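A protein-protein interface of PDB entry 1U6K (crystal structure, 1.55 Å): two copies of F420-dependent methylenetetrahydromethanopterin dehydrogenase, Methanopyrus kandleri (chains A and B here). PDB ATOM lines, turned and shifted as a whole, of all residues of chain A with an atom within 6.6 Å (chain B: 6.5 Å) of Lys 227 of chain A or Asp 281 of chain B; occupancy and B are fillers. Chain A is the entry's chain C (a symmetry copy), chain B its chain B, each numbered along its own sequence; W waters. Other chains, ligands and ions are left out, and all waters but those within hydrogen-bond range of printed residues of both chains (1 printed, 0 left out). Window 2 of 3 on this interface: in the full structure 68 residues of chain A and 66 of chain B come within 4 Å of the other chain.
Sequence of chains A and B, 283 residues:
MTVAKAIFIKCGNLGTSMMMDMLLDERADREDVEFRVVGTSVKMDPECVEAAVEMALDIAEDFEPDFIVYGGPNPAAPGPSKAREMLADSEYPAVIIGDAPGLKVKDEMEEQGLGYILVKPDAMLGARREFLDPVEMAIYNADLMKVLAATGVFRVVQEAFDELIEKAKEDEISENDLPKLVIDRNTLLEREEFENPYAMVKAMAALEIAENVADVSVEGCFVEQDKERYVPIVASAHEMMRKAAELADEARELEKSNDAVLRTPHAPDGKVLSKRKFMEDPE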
ATOM      1  N   GLU A 130      14.759  13.958  18.915  1.00  0.00           N
ATOM      2  CA  GLU A 130      15.763  14.725  19.603  1.00  0.00           C
ATOM      3  C   GLU A 130      17.143  14.098  19.541  1.00  0.00           C
ATOM      4  O   GLU A 130      18.152  14.742  19.873  1.00  0.00           O
ATOM      5  CB  GLU A 130      15.380  14.888  21.062  1.00  0.00           C
ATOM      6  CG  GLU A 130      14.052  15.618  21.270  1.00  0.00           C
ATOM      7  CD  GLU A 130      12.889  14.681  21.461  1.00  0.00           C
ATOM      8  OE1 GLU A 130      11.945  15.065  22.198  1.00  0.00           O
ATOM      9  OE2 GLU A 130      12.874  13.571  20.885  1.00  0.00           O
ATOM     10  N   GLU A 224       8.506   5.602  27.922  1.00  0.00           N
ATOM     11  CA  GLU A 224       8.889   6.831  28.615  1.00  0.00           C
ATOM     12  C   GLU A 224       8.412   8.052  27.842  1.00  0.00           C
ATOM     13  O   GLU A 224       8.660   8.159  26.638  1.00  0.00           O
ATOM     14  CB  GLU A 224      10.418   6.872  28.785  1.00  0.00           C
ATOM     15  CG  GLU A 224      10.923   8.100  29.519  1.00  0.00           C
ATOM     16  CD  GLU A 224      10.304   8.266  30.904  1.00  0.00           C
ATOM     17  OE1 GLU A 224       9.487   9.206  31.086  1.00  0.00           O
ATOM     18  OE2 GLU A 224      10.633   7.462  31.812  1.00  0.00           O
ATOM     19  N   GLN A 225       7.719   8.960  28.536  1.00  0.00           N
ATOM     20  CA  GLN A 225       7.170  10.162  27.922  1.00  0.00           C
ATOM     21  C   GLN A 225       7.860  11.468  28.313  1.00  0.00           C
ATOM     22  O   GLN A 225       7.604  12.521  27.706  1.00  0.00           O
ATOM     23  CB  GLN A 225       5.676  10.258  28.263  1.00  0.00           C
ATOM     24  CG  GLN A 225       4.858   9.055  27.795  1.00  0.00           C
ATOM     25  CD  GLN A 225       4.868   8.907  26.292  1.00  0.00           C
ATOM     26  OE1 GLN A 225       4.518   9.840  25.566  1.00  0.00           O
ATOM     27  NE2 GLN A 225       5.272   7.736  25.810  1.00  0.00           N
ATOM     28  N   ASP A 226       8.716  11.428  29.329  1.00  0.00           N
ATOM     29  CA  ASP A 226       9.448  12.620  29.754  1.00  0.00           C
ATOM     30  C   ASP A 226      10.747  12.690  28.927  1.00  0.00           C
ATOM     31  O   ASP A 226      11.596  11.811  29.054  1.00  0.00           O
ATOM     32  CB  ASP A 226       9.760  12.508  31.261  1.00  0.00           C
ATOM     33  CG  ASP A 226      10.573  13.681  31.782  1.00  0.00           C
ATOM     34  OD1 ASP A 226      10.846  13.744  33.004  1.00  0.00           O
ATOM     35  OD2 ASP A 226      10.943  14.551  30.974  1.00  0.00           O
ATOM     36  N   LYS A 227      10.897  13.700  28.071  1.00  0.00           N
ATOM     37  CA  LYS A 227      12.102  13.849  27.233  1.00  0.00           C
ATOM     38  C   LYS A 227      13.400  13.866  28.042  1.00  0.00           C
ATOM     39  O   LYS A 227      14.461  13.515  27.505  1.00  0.00           O
ATOM     40  CB  LYS A 227      12.077  15.158  26.433  1.00  0.00           C
ATOM     41  CG  LYS A 227      12.466  16.380  27.285  1.00  0.00           C
ATOM     42  CD  LYS A 227      12.586  17.689  26.480  1.00  0.00           C
ATOM     43  CE  LYS A 227      11.604  17.738  25.327  1.00  0.00           C
ATOM     44  NZ  LYS A 227      11.454  19.120  24.750  1.00  0.00           N
ATOM     45  N   GLU A 228      13.347  14.312  29.296  1.00  0.00           N
ATOM     46  CA  GLU A 228      14.568  14.359  30.099  1.00  0.00           C
ATOM     47  C   GLU A 228      15.060  12.959  30.434  1.00  0.00           C
ATOM     48  O   GLU A 228      16.222  12.765  30.840  1.00  0.00           O
ATOM     49  CB  GLU A 228      14.345  15.156  31.382  1.00  0.00           C
ATOM     50  CG  GLU A 228      14.217  16.650  31.125  1.00  0.00           C
ATOM     51  CD  GLU A 228      14.386  17.477  32.387  1.00  0.00           C
ATOM     52  OE1 GLU A 228      14.580  18.706  32.264  1.00  0.00           O
ATOM     53  OE2 GLU A 228      14.322  16.901  33.500  1.00  0.00           O
ATOM     54  N   ARG A 229      14.168  11.992  30.271  1.00  0.00           N
ATOM     55  CA  ARG A 229      14.512  10.601  30.547  1.00  0.00           C
ATOM     56  C   ARG A 229      14.622   9.824  29.228  1.00  0.00           C
ATOM     57  O   ARG A 229      15.586   9.094  29.024  1.00  0.00           O
ATOM     58  CB  ARG A 229      13.459   9.949  31.450  1.00  0.00           C
ATOM     59  CG  ARG A 229      13.465  10.471  32.895  1.00  0.00           C
ATOM     60  CD  ARG A 229      12.235   9.940  33.644  1.00  0.00           C
ATOM     61  NE  ARG A 229      12.330   8.503  33.898  1.00  0.00           N
ATOM     62  CZ  ARG A 229      12.981   7.988  34.939  1.00  0.00           C
ATOM     63  NH1 ARG A 229      13.034   6.663  35.098  1.00  0.00           N
ATOM     64  NH2 ARG A 229      13.562   8.797  35.828  1.00  0.00           N
ATOM     65  N   TYR A 230      13.688  10.001  28.291  1.00  0.00           N
ATOM     66  CA  TYR A 230      13.802   9.211  27.060  1.00  0.00           C
ATOM     67  C   TYR A 230      14.956   9.524  26.096  1.00  0.00           C
ATOM     68  O   TYR A 230      15.368   8.622  25.362  1.00  0.00           O
ATOM     69  CB  TYR A 230      12.466   9.126  26.264  1.00  0.00           C
ATOM     70  CG  TYR A 230      11.940  10.378  25.595  1.00  0.00           C
ATOM     71  CD1 TYR A 230      10.722  10.949  26.007  1.00  0.00           C
ATOM     72  CD2 TYR A 230      12.597  10.949  24.523  1.00  0.00           C
ATOM     73  CE1 TYR A 230      10.189  12.067  25.347  1.00  0.00           C
ATOM     74  CE2 TYR A 230      12.075  12.060  23.854  1.00  0.00           C
ATOM     75  CZ  TYR A 230      10.865  12.611  24.279  1.00  0.00           C
ATOM     76  OH  TYR A 230      10.336  13.710  23.624  1.00  0.00           O
ATOM     77  N   VAL A 231      15.473  10.760  26.068  1.00  0.00           N
ATOM     78  CA  VAL A 231      16.589  11.051  25.157  1.00  0.00           C
ATOM     79  C   VAL A 231      17.816  10.260  25.702  1.00  0.00           C
ATOM     80  O   VAL A 231      18.480   9.590  24.933  1.00  0.00           O
ATOM     81  CB  VAL A 231      16.846  12.568  25.041  1.00  0.00           C
ATOM     82  CG1 VAL A 231      18.066  12.852  24.212  1.00  0.00           C
ATOM     83  CG2 VAL A 231      15.623  13.216  24.378  1.00  0.00           C
ATOM     84  N   PRO A 232      18.107  10.344  27.013  1.00  0.00           N
ATOM     85  CA  PRO A 232      19.249   9.558  27.522  1.00  0.00           C
ATOM     86  C   PRO A 232      19.010   8.057  27.296  1.00  0.00           C
ATOM     87  O   PRO A 232      19.940   7.305  26.951  1.00  0.00           O
ATOM     88  CB  PRO A 232      19.267   9.886  29.004  1.00  0.00           C
ATOM     89  CG  PRO A 232      18.801  11.299  29.037  1.00  0.00           C
ATOM     90  CD  PRO A 232      17.741  11.404  27.977  1.00  0.00           C
ATOM     91  N   SER B 274      18.070  21.635  13.816  1.00  0.00           N
ATOM     92  CA  SER B 274      19.475  21.560  14.196  1.00  0.00           C
ATOM     93  C   SER B 274      19.634  21.675  15.699  1.00  0.00           C
ATOM     94  O   SER B 274      18.837  22.327  16.366  1.00  0.00           O
ATOM     95  CB  SER B 274      20.255  22.691  13.516  1.00  0.00           C
ATOM     96  OG  SER B 274      21.637  22.690  13.864  1.00  0.00           O
ATOM     97  N   LYS B 275      20.674  21.034  16.235  1.00  0.00           N
ATOM     98  CA  LYS B 275      20.976  21.111  17.658  1.00  0.00           C
ATOM     99  C   LYS B 275      22.433  20.655  17.841  1.00  0.00           C
ATOM    100  O   LYS B 275      22.982  19.963  16.972  1.00  0.00           O
ATOM    101  CB  LYS B 275      20.058  20.202  18.479  1.00  0.00           C
ATOM    102  CG  LYS B 275      20.096  18.709  18.083  1.00  0.00           C
ATOM    103  CD  LYS B 275      19.272  17.835  19.027  1.00  0.00           C
ATOM    104  CE  LYS B 275      20.022  17.501  20.344  1.00  0.00           C
ATOM    105  NZ  LYS B 275      19.163  16.806  21.343  1.00  0.00           N
ATOM    106  N   LYS B 277      23.852  20.566  21.666  1.00  0.00           N
ATOM    107  CA  LYS B 277      23.915  19.987  23.011  1.00  0.00           C
ATOM    108  C   LYS B 277      22.977  18.807  23.128  1.00  0.00           C
ATOM    109  O   LYS B 277      21.867  18.801  22.588  1.00  0.00           O
ATOM    110  CB  LYS B 277      23.592  21.025  24.083  1.00  0.00           C
ATOM    111  CG  LYS B 277      24.650  22.117  24.226  1.00  0.00           C
ATOM    112  CD  LYS B 277      24.440  22.881  25.532  1.00  0.00           C
ATOM    113  CE  LYS B 277      25.660  23.729  25.880  1.00  0.00           C
ATOM    114  NZ  LYS B 277      26.863  22.880  26.169  1.00  0.00           N
ATOM    115  N   PHE B 278      23.404  17.795  23.875  1.00  0.00           N
ATOM    116  CA  PHE B 278      22.599  16.609  23.975  1.00  0.00           C
ATOM    117  C   PHE B 278      21.156  16.831  24.417  1.00  0.00           C
ATOM    118  O   PHE B 278      20.239  16.235  23.848  1.00  0.00           O
ATOM    119  CB  PHE B 278      23.287  15.623  24.929  1.00  0.00           C
ATOM    120  CG  PHE B 278      22.609  14.283  25.025  1.00  0.00           C
ATOM    121  CD1 PHE B 278      21.927  13.914  26.185  1.00  0.00           C
ATOM    122  CD2 PHE B 278      22.652  13.391  23.954  1.00  0.00           C
ATOM    123  CE1 PHE B 278      21.293  12.670  26.276  1.00  0.00           C
ATOM    124  CE2 PHE B 278      22.016  12.144  24.028  1.00  0.00           C
ATOM    125  CZ  PHE B 278      21.339  11.785  25.189  1.00  0.00           C
ATOM    126  N   MET B 279      20.972  17.677  25.424  1.00  0.00           N
ATOM    127  CA  MET B 279      19.629  17.915  25.947  1.00  0.00           C
ATOM    128  C   MET B 279      18.899  19.093  25.332  1.00  0.00           C
ATOM    129  O   MET B 279      17.836  19.476  25.803  1.00  0.00           O
ATOM    130  CB  MET B 279      19.677  18.084  27.462  1.00  0.00           C
ATOM    131  CG  MET B 279      20.282  16.898  28.207  1.00  0.00           C
ATOM    132  SD  MET B 279      19.287  15.192  28.208  1.00  0.00           S
ATOM    133  CE  MET B 279      18.020  15.464  26.881  1.00  0.00           C
ATOM    134  N   GLU B 280      19.458  19.639  24.272  1.00  0.00           N
ATOM    135  CA  GLU B 280      18.895  20.787  23.560  1.00  0.00           C
ATOM    136  C   GLU B 280      17.836  20.329  22.541  1.00  0.00           C
ATOM    137  O   GLU B 280      18.084  19.415  21.753  1.00  0.00           O
ATOM    138  CB  GLU B 280      20.059  21.462  22.851  1.00  0.00           C
ATOM    139  CG  GLU B 280      19.796  22.703  22.065  1.00  0.00           C
ATOM    140  CD  GLU B 280      20.896  22.911  21.038  1.00  0.00           C
ATOM    141  OE1 GLU B 280      22.035  22.430  21.267  1.00  0.00           O
ATOM    142  OE2 GLU B 280      20.629  23.579  20.010  1.00  0.00           O
ATOM    143  N   ASP B 281      16.649  20.934  22.556  1.00  0.00           N
ATOM    144  CA  ASP B 281      15.635  20.552  21.575  1.00  0.00           C
ATOM    145  C   ASP B 281      16.099  21.035  20.202  1.00  0.00           C
ATOM    146  O   ASP B 281      16.676  22.118  20.082  1.00  0.00           O
ATOM    147  CB  ASP B 281      14.271  21.205  21.876  1.00  0.00           C
ATOM    148  CG  ASP B 281      13.437  20.414  22.873  1.00  0.00           C
ATOM    149  OD1 ASP B 281      13.641  19.186  23.011  1.00  0.00           O
ATOM    150  OD2 ASP B 281      12.550  21.027  23.505  1.00  0.00           O
ATOM    151  N   PRO B 282      15.873  20.234  19.151  1.00  0.00           N
ATOM    152  CA  PRO B 282      16.281  20.635  17.800  1.00  0.00           C
ATOM    153  C   PRO B 282      15.307  21.691  17.255  1.00  0.00           C
ATOM    154  O   PRO B 282      14.087  21.505  17.324  1.00  0.00           O
ATOM    155  CB  PRO B 282      16.224  19.333  17.016  1.00  0.00           C
ATOM    156  CG  PRO B 282      15.161  18.548  17.738  1.00  0.00           C
ATOM    157  CD  PRO B 282      15.400  18.837  19.176  1.00  0.00           C
ATOM    158  N   GLU B 283      15.850  22.779  16.723  1.00  0.00           N
ATOM    159  CA  GLU B 283      15.028  23.865  16.187  1.00  0.00           C
ATOM    160  C   GLU B 283      15.219  23.990  14.681  1.00  0.00           C
ATOM    161  O   GLU B 283      14.217  24.175  13.988  1.00  0.00           O
ATOM    162  CB  GLU B 283      15.401  25.204  16.836  1.00  0.00           C
ATOM    163  CG  GLU B 283      15.520  25.196  18.353  1.00  0.00           C
ATOM    164  CD  GLU B 283      14.212  24.895  19.052  1.00  0.00           C
ATOM    165  OE1 GLU B 283      13.647  23.808  18.813  1.00  0.00           O
ATOM    166  OE2 GLU B 283      13.752  25.747  19.845  1.00  0.00           O
ATOM    167  OXT GLU B 283      16.327  24.049  14.243  1.00  0.00           O
HETATM  168  O   HOH W   1      11.460  17.735  22.021  1.00  0.00           O
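The side-chain amino group (NZ) of Lys 275 of chain B sits at hydrogen-bond distance from the backbone carbonyl oxygen (O) of Glu 130 of chain A, 2.7 Å away. NZ of Lys 227 of chain A is in salt-bridge range of OD2 of Asp 281 of chain B, at 2.5 Å.
The side-chain amino group (NZ) of Lys 275 of chain B lies within hydrogen-bond range of the backbone carbonyl oxygen (O) of Phe 278 of chain B (2.8 Å). NZ of Lys 275 of chain B is in hydrogen-bond range of O of Glu 280 of chain B (2.9 Å). OH of Tyr 230 of chain A sits at hydrogen-bond distance from OE1 of Glu 130 of chain A (2.5 Å).
Among the printed residues, merely in contact across the chains: Val 231 of chain A with Phe 278 of chain B, Val 231 of chain A with Met 279 of chain B, Pro 232 of chain A with Phe 278 of chain B and Glu 130 of chain A with Asp 281 of chain B.
Asp 226 of chain A touches none of the printed residues of chain B. Of the printed residues of chain B, Lys 227 of chain A touches Asp 281. Printed residues of chain B within 4 Å of Val 231 of chain A: Phe 278 (3.6 Å) and Met 279 (3.6 Å). Of the printed residues of chain B, Pro 232 of chain A touches Phe 278 (3.8 Å). Ser 274 of chain B touches none of the printed residues of chain A. Of the printed residues of chain A, Asp 281 of chain B touches Glu 130 and Lys 227. The nearest residue of chain B that does not touch Lys 227 of chain A is Met 279 of chain B (4.1 Å). The nearest printed residue of chain A that does not touch Met 279 of chain B is Pro 232 of chain A (4.01 Å).
Hydrophobic or aromatic side chains of chain A that line the printed part of chain B: Val 231 and Pro 232. Along chain A the printed residues that touch a printed residue of chain B span positions 130 to 232. Among the printed residues, Asp or Glu carboxylates within 4 Å of a Lys or Arg side-chain nitrogen of the other chain: Lys 227 of chain A with Asp 281 of chain B.
No position is printed for both chains. Of the 6 pairs that touch across the chains among the printed residues, none has its exchanged pair printed and touching as well.
Water W1 lies within hydrogen-bond range of OE1 of Glu 130 of chain A (2.7 Å), OD1 of Asp 281 of chain B (2.8 Å) and NZ of Lys 227 of chain A (3.1 Å).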
